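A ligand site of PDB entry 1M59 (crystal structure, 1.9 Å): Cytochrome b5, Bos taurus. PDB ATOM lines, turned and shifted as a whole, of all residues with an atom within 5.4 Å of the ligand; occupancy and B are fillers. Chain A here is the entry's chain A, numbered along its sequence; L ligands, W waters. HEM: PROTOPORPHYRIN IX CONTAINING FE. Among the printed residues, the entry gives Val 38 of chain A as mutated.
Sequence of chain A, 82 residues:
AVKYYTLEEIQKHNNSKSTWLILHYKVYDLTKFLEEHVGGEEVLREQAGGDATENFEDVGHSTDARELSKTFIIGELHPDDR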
ATOM      1  N   LEU A  21       6.328 -13.161  -5.801  1.00  0.00           N
ATOM      2  CA  LEU A  21       6.783 -11.867  -6.267  1.00  0.00           C
ATOM      3  C   LEU A  21       8.303 -11.841  -6.215  1.00  0.00           C
ATOM      4  O   LEU A  21       8.928 -12.690  -5.567  1.00  0.00           O
ATOM      5  CB  LEU A  21       6.142 -10.715  -5.494  1.00  0.00           C
ATOM      6  CG  LEU A  21       6.173 -10.587  -3.983  1.00  0.00           C
ATOM      7  CD1 LEU A  21       7.580 -10.207  -3.512  1.00  0.00           C
ATOM      8  CD2 LEU A  21       5.183  -9.511  -3.576  1.00  0.00           C
ATOM      9  N   LEU A  23      11.926  -9.745  -5.503  1.00  0.00           N
ATOM     10  CA  LEU A  23      12.554  -8.670  -4.759  1.00  0.00           C
ATOM     11  C   LEU A  23      14.057  -8.845  -4.972  1.00  0.00           C
ATOM     12  O   LEU A  23      14.631  -9.854  -4.549  1.00  0.00           O
ATOM     13  CB  LEU A  23      12.225  -8.741  -3.257  1.00  0.00           C
ATOM     14  CG  LEU A  23      10.783  -8.515  -2.801  1.00  0.00           C
ATOM     15  CD1 LEU A  23      10.688  -8.735  -1.297  1.00  0.00           C
ATOM     16  CD2 LEU A  23      10.321  -7.110  -3.148  1.00  0.00           C
ATOM     17  N   TYR A  28      10.048 -14.816  -4.006  1.00  0.00           N
ATOM     18  CA  TYR A  28       9.465 -15.102  -2.703  1.00  0.00           C
ATOM     19  C   TYR A  28       8.072 -15.678  -2.815  1.00  0.00           C
ATOM     20  O   TYR A  28       7.268 -15.196  -3.624  1.00  0.00           O
ATOM     21  CB  TYR A  28       9.380 -13.831  -1.851  1.00  0.00           C
ATOM     22  CG  TYR A  28      10.696 -13.173  -1.542  1.00  0.00           C
ATOM     23  CD1 TYR A  28      11.451 -12.567  -2.553  1.00  0.00           C
ATOM     24  CD2 TYR A  28      11.211 -13.163  -0.240  1.00  0.00           C
ATOM     25  CE1 TYR A  28      12.675 -11.966  -2.268  1.00  0.00           C
ATOM     26  CE2 TYR A  28      12.438 -12.556   0.052  1.00  0.00           C
ATOM     27  CZ  TYR A  28      13.165 -11.964  -0.981  1.00  0.00           C
ATOM     28  OH  TYR A  28      14.370 -11.365  -0.716  1.00  0.00           O
ATOM     29  N   LEU A  30       4.931 -15.739  -0.960  1.00  0.00           N
ATOM     30  CA  LEU A  30       4.289 -15.102   0.196  1.00  0.00           C
ATOM     31  C   LEU A  30       2.861 -15.553   0.447  1.00  0.00           C
ATOM     32  O   LEU A  30       2.122 -14.894   1.179  1.00  0.00           O
ATOM     33  CB  LEU A  30       4.294 -13.586   0.005  1.00  0.00           C
ATOM     34  CG  LEU A  30       5.658 -12.904  -0.142  1.00  0.00           C
ATOM     35  CD1 LEU A  30       5.452 -11.391  -0.245  1.00  0.00           C
ATOM     36  CD2 LEU A  30       6.535 -13.231   1.059  1.00  0.00           C
ATOM     37  N   PHE A  33       2.014 -15.783   4.083  1.00  0.00           N
ATOM     38  CA  PHE A  33       2.397 -14.583   4.808  1.00  0.00           C
ATOM     39  C   PHE A  33       1.401 -13.433   4.640  1.00  0.00           C
ATOM     40  O   PHE A  33       1.336 -12.538   5.474  1.00  0.00           O
ATOM     41  CB  PHE A  33       3.784 -14.141   4.341  1.00  0.00           C
ATOM     42  CG  PHE A  33       4.282 -12.902   5.009  1.00  0.00           C
ATOM     43  CD1 PHE A  33       4.477 -11.728   4.282  1.00  0.00           C
ATOM     44  CD2 PHE A  33       4.593 -12.920   6.365  1.00  0.00           C
ATOM     45  CE1 PHE A  33       4.966 -10.584   4.898  1.00  0.00           C
ATOM     46  CE2 PHE A  33       5.084 -11.770   6.989  1.00  0.00           C
ATOM     47  CZ  PHE A  33       5.270 -10.613   6.252  1.00  0.00           C
ATOM     48  N   HIS A  37       1.311 -10.088   7.322  1.00  0.00           N
ATOM     49  CA  HIS A  37       1.999  -8.848   6.950  1.00  0.00           C
ATOM     50  C   HIS A  37       1.365  -7.668   7.673  1.00  0.00           C
ATOM     51  O   HIS A  37       0.184  -7.374   7.460  1.00  0.00           O
ATOM     52  CB  HIS A  37       1.875  -8.663   5.445  1.00  0.00           C
ATOM     53  CG  HIS A  37       2.648  -7.492   4.914  1.00  0.00           C
ATOM     54  ND1 HIS A  37       2.183  -6.662   3.922  1.00  0.00           N
ATOM     55  CD2 HIS A  37       3.904  -7.069   5.203  1.00  0.00           C
ATOM     56  CE1 HIS A  37       3.140  -5.775   3.651  1.00  0.00           C
ATOM     57  NE2 HIS A  37       4.209  -5.983   4.405  1.00  0.00           N
ATOM     58  N   VAL A  38       2.118  -6.960   8.523  1.00  0.00           N
ATOM     59  CA  VAL A  38       1.542  -5.830   9.234  1.00  0.00           C
ATOM     60  C   VAL A  38       1.155  -4.700   8.259  1.00  0.00           C
ATOM     61  O   VAL A  38       0.328  -3.850   8.575  1.00  0.00           O
ATOM     62  CB  VAL A  38       2.787  -5.387   9.990  1.00  0.00           C
ATOM     63  CG1 VAL A  38       2.446  -4.033  10.601  1.00  0.00           C
ATOM     64  CG2 VAL A  38       2.996  -6.426  11.024  1.00  0.00           C
ATOM     65  N   GLY A  39       1.762  -4.721   7.077  1.00  0.00           N
ATOM     66  CA  GLY A  39       1.462  -3.715   6.076  1.00  0.00           C
ATOM     67  C   GLY A  39       0.224  -4.043   5.255  1.00  0.00           C
ATOM     68  O   GLY A  39      -0.113  -3.332   4.314  1.00  0.00           O
ATOM     69  N   VAL A  43      -1.617  -4.708  -0.423  1.00  0.00           N
ATOM     70  CA  VAL A  43      -0.412  -4.212  -1.074  1.00  0.00           C
ATOM     71  C   VAL A  43       0.428  -5.336  -1.668  1.00  0.00           C
ATOM     72  O   VAL A  43       1.179  -5.128  -2.623  1.00  0.00           O
ATOM     73  CB  VAL A  43       0.448  -3.383  -0.071  1.00  0.00           C
ATOM     74  CG1 VAL A  43       1.021  -4.291   1.011  1.00  0.00           C
ATOM     75  CG2 VAL A  43       1.553  -2.664  -0.812  1.00  0.00           C
ATOM     76  N   LEU A  44       0.313  -6.540  -1.116  1.00  0.00           N
ATOM     77  CA  LEU A  44       1.067  -7.683  -1.624  1.00  0.00           C
ATOM     78  C   LEU A  44       0.358  -8.279  -2.845  1.00  0.00           C
ATOM     79  O   LEU A  44       1.000  -8.588  -3.859  1.00  0.00           O
ATOM     80  CB  LEU A  44       1.233  -8.740  -0.527  1.00  0.00           C
ATOM     81  CG  LEU A  44       2.003  -8.250   0.713  1.00  0.00           C
ATOM     82  CD1 LEU A  44       2.077  -9.360   1.755  1.00  0.00           C
ATOM     83  CD2 LEU A  44       3.397  -7.829   0.299  1.00  0.00           C
ATOM     84  N   GLN A  47       1.004  -6.616  -6.184  1.00  0.00           N
ATOM     85  CA  GLN A  47       2.320  -6.818  -6.786  1.00  0.00           C
ATOM     86  C   GLN A  47       2.555  -8.270  -7.205  1.00  0.00           C
ATOM     87  O   GLN A  47       3.562  -8.571  -7.854  1.00  0.00           O
ATOM     88  CB  GLN A  47       3.416  -6.377  -5.815  1.00  0.00           C
ATOM     89  CG  GLN A  47       3.351  -4.916  -5.416  1.00  0.00           C
ATOM     90  CD  GLN A  47       3.407  -3.972  -6.603  1.00  0.00           C
ATOM     91  OE1 GLN A  47       4.333  -4.033  -7.411  1.00  0.00           O
ATOM     92  NE2 GLN A  47       2.410  -3.097  -6.709  1.00  0.00           N
ATOM     93  N   ALA A  52       8.490  -6.369  -7.312  1.00  0.00           N
ATOM     94  CA  ALA A  52       8.023  -5.348  -6.371  1.00  0.00           C
ATOM     95  C   ALA A  52       9.175  -4.701  -5.600  1.00  0.00           C
ATOM     96  O   ALA A  52       8.954  -4.148  -4.525  1.00  0.00           O
ATOM     97  CB  ALA A  52       7.041  -5.961  -5.393  1.00  0.00           C
ATOM     98  N   ASN A  55       8.787  -0.732  -4.874  1.00  0.00           N
ATOM     99  CA  ASN A  55       7.738  -0.498  -3.891  1.00  0.00           C
ATOM    100  C   ASN A  55       8.186  -0.935  -2.506  1.00  0.00           C
ATOM    101  O   ASN A  55       7.880  -0.296  -1.492  1.00  0.00           O
ATOM    102  CB  ASN A  55       6.469  -1.238  -4.289  1.00  0.00           C
ATOM    103  CG  ASN A  55       6.006  -0.889  -5.691  1.00  0.00           C
ATOM    104  OD1 ASN A  55       6.330  -1.589  -6.647  1.00  0.00           O
ATOM    105  ND2 ASN A  55       5.244   0.188  -5.816  1.00  0.00           N
ATOM    106  N   PHE A  56       8.924  -2.045  -2.454  1.00  0.00           N
ATOM    107  CA  PHE A  56       9.435  -2.599  -1.211  1.00  0.00           C
ATOM    108  C   PHE A  56      10.431  -1.640  -0.561  1.00  0.00           C
ATOM    109  O   PHE A  56      10.401  -1.414   0.652  1.00  0.00           O
ATOM    110  CB  PHE A  56      10.113  -3.936  -1.509  1.00  0.00           C
ATOM    111  CG  PHE A  56      10.701  -4.614  -0.301  1.00  0.00           C
ATOM    112  CD1 PHE A  56       9.879  -5.296   0.605  1.00  0.00           C
ATOM    113  CD2 PHE A  56      12.065  -4.574  -0.057  1.00  0.00           C
ATOM    114  CE1 PHE A  56      10.420  -5.933   1.725  1.00  0.00           C
ATOM    115  CE2 PHE A  56      12.612  -5.205   1.058  1.00  0.00           C
ATOM    116  CZ  PHE A  56      11.793  -5.887   1.950  1.00  0.00           C
ATOM    117  N   VAL A  59       9.012   2.004   0.810  1.00  0.00           N
ATOM    118  CA  VAL A  59       8.431   2.060   2.152  1.00  0.00           C
ATOM    119  C   VAL A  59       9.499   1.902   3.242  1.00  0.00           C
ATOM    120  O   VAL A  59       9.214   2.061   4.423  1.00  0.00           O
ATOM    121  CB  VAL A  59       7.336   0.994   2.336  1.00  0.00           C
ATOM    122  CG1 VAL A  59       6.352   1.045   1.183  1.00  0.00           C
ATOM    123  CG2 VAL A  59       7.961  -0.370   2.420  1.00  0.00           C
ATOM    124  N   GLY A  60      10.723   1.567   2.830  1.00  0.00           N
ATOM    125  CA  GLY A  60      11.822   1.406   3.759  1.00  0.00           C
ATOM    126  C   GLY A  60      11.761   0.390   4.888  1.00  0.00           C
ATOM    127  O   GLY A  60      11.841   0.754   6.071  1.00  0.00           O
ATOM    128  N   HIS A  61      11.634  -0.888   4.543  1.00  0.00           N
ATOM    129  CA  HIS A  61      11.487  -1.948   5.531  1.00  0.00           C
ATOM    130  C   HIS A  61      12.640  -2.041   6.512  1.00  0.00           C
ATOM    131  O   HIS A  61      13.803  -1.944   6.134  1.00  0.00           O
ATOM    132  CB  HIS A  61      11.323  -3.308   4.832  1.00  0.00           C
ATOM    133  CG  HIS A  61       9.960  -3.515   4.253  1.00  0.00           C
ATOM    134  ND1 HIS A  61       9.530  -2.961   3.069  1.00  0.00           N
ATOM    135  CD2 HIS A  61       8.912  -4.222   4.738  1.00  0.00           C
ATOM    136  CE1 HIS A  61       8.258  -3.341   2.893  1.00  0.00           C
ATOM    137  NE2 HIS A  61       7.841  -4.097   3.882  1.00  0.00           N
ATOM    138  N   SER A  62      12.308  -2.258   7.781  1.00  0.00           N
ATOM    139  CA  SER A  62      13.314  -2.374   8.838  1.00  0.00           C
ATOM    140  C   SER A  62      14.218  -3.576   8.615  1.00  0.00           C
ATOM    141  O   SER A  62      13.937  -4.438   7.780  1.00  0.00           O
ATOM    142  CB  SER A  62      12.629  -2.491  10.198  1.00  0.00           C
ATOM    143  OG  SER A  62      11.828  -3.666  10.260  1.00  0.00           O
ATOM    144  N   ALA A  65      12.421  -6.924   9.351  1.00  0.00           N
ATOM    145  CA  ALA A  65      11.534  -7.386   8.285  1.00  0.00           C
ATOM    146  C   ALA A  65      12.338  -8.025   7.159  1.00  0.00           C
ATOM    147  O   ALA A  65      11.944  -9.063   6.619  1.00  0.00           O
ATOM    148  CB  ALA A  65      10.717  -6.220   7.740  1.00  0.00           C
ATOM    149  N   LEU A  68      13.547 -11.464   8.134  1.00  0.00           N
ATOM    150  CA  LEU A  68      12.451 -12.415   8.110  1.00  0.00           C
ATOM    151  C   LEU A  68      12.083 -12.819   6.686  1.00  0.00           C
ATOM    152  O   LEU A  68      11.788 -13.983   6.417  1.00  0.00           O
ATOM    153  CB  LEU A  68      11.222 -11.830   8.803  1.00  0.00           C
ATOM    154  CG  LEU A  68       9.934 -12.671   8.710  1.00  0.00           C
ATOM    155  CD1 LEU A  68      10.162 -14.028   9.344  1.00  0.00           C
ATOM    156  CD2 LEU A  68       8.802 -11.936   9.405  1.00  0.00           C
ATOM    157  N   SER A  69      12.106 -11.845   5.768  1.00  0.00           N
ATOM    158  CA  SER A  69      11.755 -12.115   4.376  1.00  0.00           C
ATOM    159  C   SER A  69      12.547 -13.265   3.762  1.00  0.00           C
ATOM    160  O   SER A  69      12.042 -13.961   2.885  1.00  0.00           O
ATOM    161  CB  SER A  69      11.955 -10.857   3.517  1.00  0.00           C
ATOM    162  OG  SER A  69      13.330 -10.581   3.313  1.00  0.00           O
ATOM    163  N   PHE A  72      11.113 -16.843   3.135  1.00  0.00           N
ATOM    164  CA  PHE A  72      10.179 -17.089   2.037  1.00  0.00           C
ATOM    165  C   PHE A  72      10.804 -17.231   0.649  1.00  0.00           C
ATOM    166  O   PHE A  72      10.095 -17.437  -0.336  1.00  0.00           O
ATOM    167  CB  PHE A  72       9.129 -15.967   1.994  1.00  0.00           C
ATOM    168  CG  PHE A  72       8.406 -15.769   3.295  1.00  0.00           C
ATOM    169  CD1 PHE A  72       7.647 -16.794   3.850  1.00  0.00           C
ATOM    170  CD2 PHE A  72       8.500 -14.564   3.977  1.00  0.00           C
ATOM    171  CE1 PHE A  72       7.002 -16.624   5.077  1.00  0.00           C
ATOM    172  CE2 PHE A  72       7.854 -14.376   5.205  1.00  0.00           C
ATOM    173  CZ  PHE A  72       7.109 -15.417   5.756  1.00  0.00           C
HETATM  174  CHA HEM L   1       5.266  -2.831   6.710  1.00  0.00           C
HETATM  175  CHB HEM L   1       7.419  -7.187   6.514  1.00  0.00           C
HETATM  176  CHC HEM L   1       6.999  -7.171   1.687  1.00  0.00           C
HETATM  177  CHD HEM L   1       4.544  -2.965   1.875  1.00  0.00           C
HETATM  178  C1A HEM L   1       5.992  -3.985   7.046  1.00  0.00           C
HETATM  179  C2A HEM L   1       6.487  -4.294   8.383  1.00  0.00           C
HETATM  180  C3A HEM L   1       6.969  -5.553   8.352  1.00  0.00           C
HETATM  181  C4A HEM L   1       6.871  -5.993   6.975  1.00  0.00           C
HETATM  182  CMA HEM L   1       7.491  -6.339   9.543  1.00  0.00           C
HETATM  183  CAA HEM L   1       6.521  -3.353   9.574  1.00  0.00           C
HETATM  184  CBA HEM L   1       7.496  -2.190   9.392  1.00  0.00           C
HETATM  185  CGA HEM L   1       8.912  -2.679   9.241  1.00  0.00           C
HETATM  186  O1A HEM L   1       9.342  -3.505  10.069  1.00  0.00           O
HETATM  187  O2A HEM L   1       9.613  -2.236   8.305  1.00  0.00           O
HETATM  188  C1B HEM L   1       7.495  -7.553   5.168  1.00  0.00           C
HETATM  189  C2B HEM L   1       8.097  -8.796   4.708  1.00  0.00           C
HETATM  190  C3B HEM L   1       7.970  -8.826   3.375  1.00  0.00           C
HETATM  191  C4B HEM L   1       7.314  -7.566   2.991  1.00  0.00           C
HETATM  192  CMB HEM L   1       8.692  -9.911   5.587  1.00  0.00           C
HETATM  193  CAB HEM L   1       8.281  -9.955   2.606  1.00  0.00           C
HETATM  194  CBB HEM L   1       8.922  -9.929   1.366  1.00  0.00           C
HETATM  195  C1C HEM L   1       6.339  -6.003   1.325  1.00  0.00           C
HETATM  196  C2C HEM L   1       6.108  -5.606  -0.051  1.00  0.00           C
HETATM  197  C3C HEM L   1       5.401  -4.434  -0.029  1.00  0.00           C
HETATM  198  C4C HEM L   1       5.202  -4.113   1.393  1.00  0.00           C
HETATM  199  CMC HEM L   1       6.521  -6.419  -1.274  1.00  0.00           C
HETATM  200  CAC HEM L   1       4.949  -3.652  -1.091  1.00  0.00           C
HETATM  201  CBC HEM L   1       4.616  -4.108  -2.364  1.00  0.00           C
HETATM  202  C1D HEM L   1       4.491  -2.603   3.220  1.00  0.00           C
HETATM  203  C2D HEM L   1       3.808  -1.427   3.725  1.00  0.00           C
HETATM  204  C3D HEM L   1       4.024  -1.369   5.067  1.00  0.00           C
HETATM  205  C4D HEM L   1       4.827  -2.530   5.417  1.00  0.00           C
HETATM  206  CMD HEM L   1       2.948  -0.492   2.893  1.00  0.00           C
HETATM  207  CAD HEM L   1       3.467  -0.333   6.056  1.00  0.00           C
HETATM  208  CBD HEM L   1       4.207   0.984   6.013  1.00  0.00           C
HETATM  209  CGD HEM L   1       3.621   2.028   6.950  1.00  0.00           C
HETATM  210  O1D HEM L   1       4.087   3.191   6.921  1.00  0.00           O
HETATM  211  O2D HEM L   1       2.709   1.684   7.738  1.00  0.00           O
HETATM  212  NA  HEM L   1       6.299  -5.019   6.163  1.00  0.00           N
HETATM  213  NB  HEM L   1       7.009  -6.802   4.113  1.00  0.00           N
HETATM  214  NC  HEM L   1       5.819  -5.067   2.216  1.00  0.00           N
HETATM  215  ND  HEM L   1       5.090  -3.314   4.269  1.00  0.00           N
HETATM  216 FE   HEM L   1       6.060  -5.045   4.205  1.00  0.00          FE
HETATM  217  O   HOH W   1       9.032   0.357   7.290  1.00  0.00           O
HETATM  218  O   HOH W   2       5.488   4.150   4.021  1.00  0.00           O
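Leu 23 touches the ligand (CD1 to CBB, 3.4 Å). Phe 33 touches the ligand. CA of Gly 39 touches C3D of the ligand, at 3.6 Å. Val 43 touches the ligand. Leu 44 touches the ligand (CD2 to C2C, 3.5 Å). Gln 47 touches the ligand. Asn 55 touches the ligand (CB to CBC, 3.9 Å). Phe 56 touches the ligand (CD1 to CHC, 3.6 Å). O of Ala 65 touches CMB of the ligand, at 3.5 Å. Ser 69 touches the ligand. Of the 22 residues printed, 13 come within 4 Å of the ligand.
Water W1 lies within hydrogen-bond range of an oxygen (O2A) of the ligand (2.8 Å), the backbone carbonyl oxygen of Gly 60 (3.1 Å) and the backbone carbonyl oxygen of Val 59 (3.3 Å).
An iron atom (FE) of the ligand is bound by a ring nitrogen (NE2) of His 37 (2.1 Å). An iron atom (FE) of the ligand is bound by a ring nitrogen (NE2) of His 61 (2.0 Å). The backbone NH (N) of Ser 62 is in hydrogen-bond range of an oxygen (O2A) of the ligand (2.7 Å). OG of Ser 62 lies within hydrogen-bond range of O1A of the ligand (2.5 Å).
OG of Ser 62 is in hydrogen-bond range of N of Ala 65. ND1 of His 61 sits at hydrogen-bond distance from O of Phe 56. OE1 of Gln 47 lies close to OD1 of Asn 55, 3.2 Å away.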
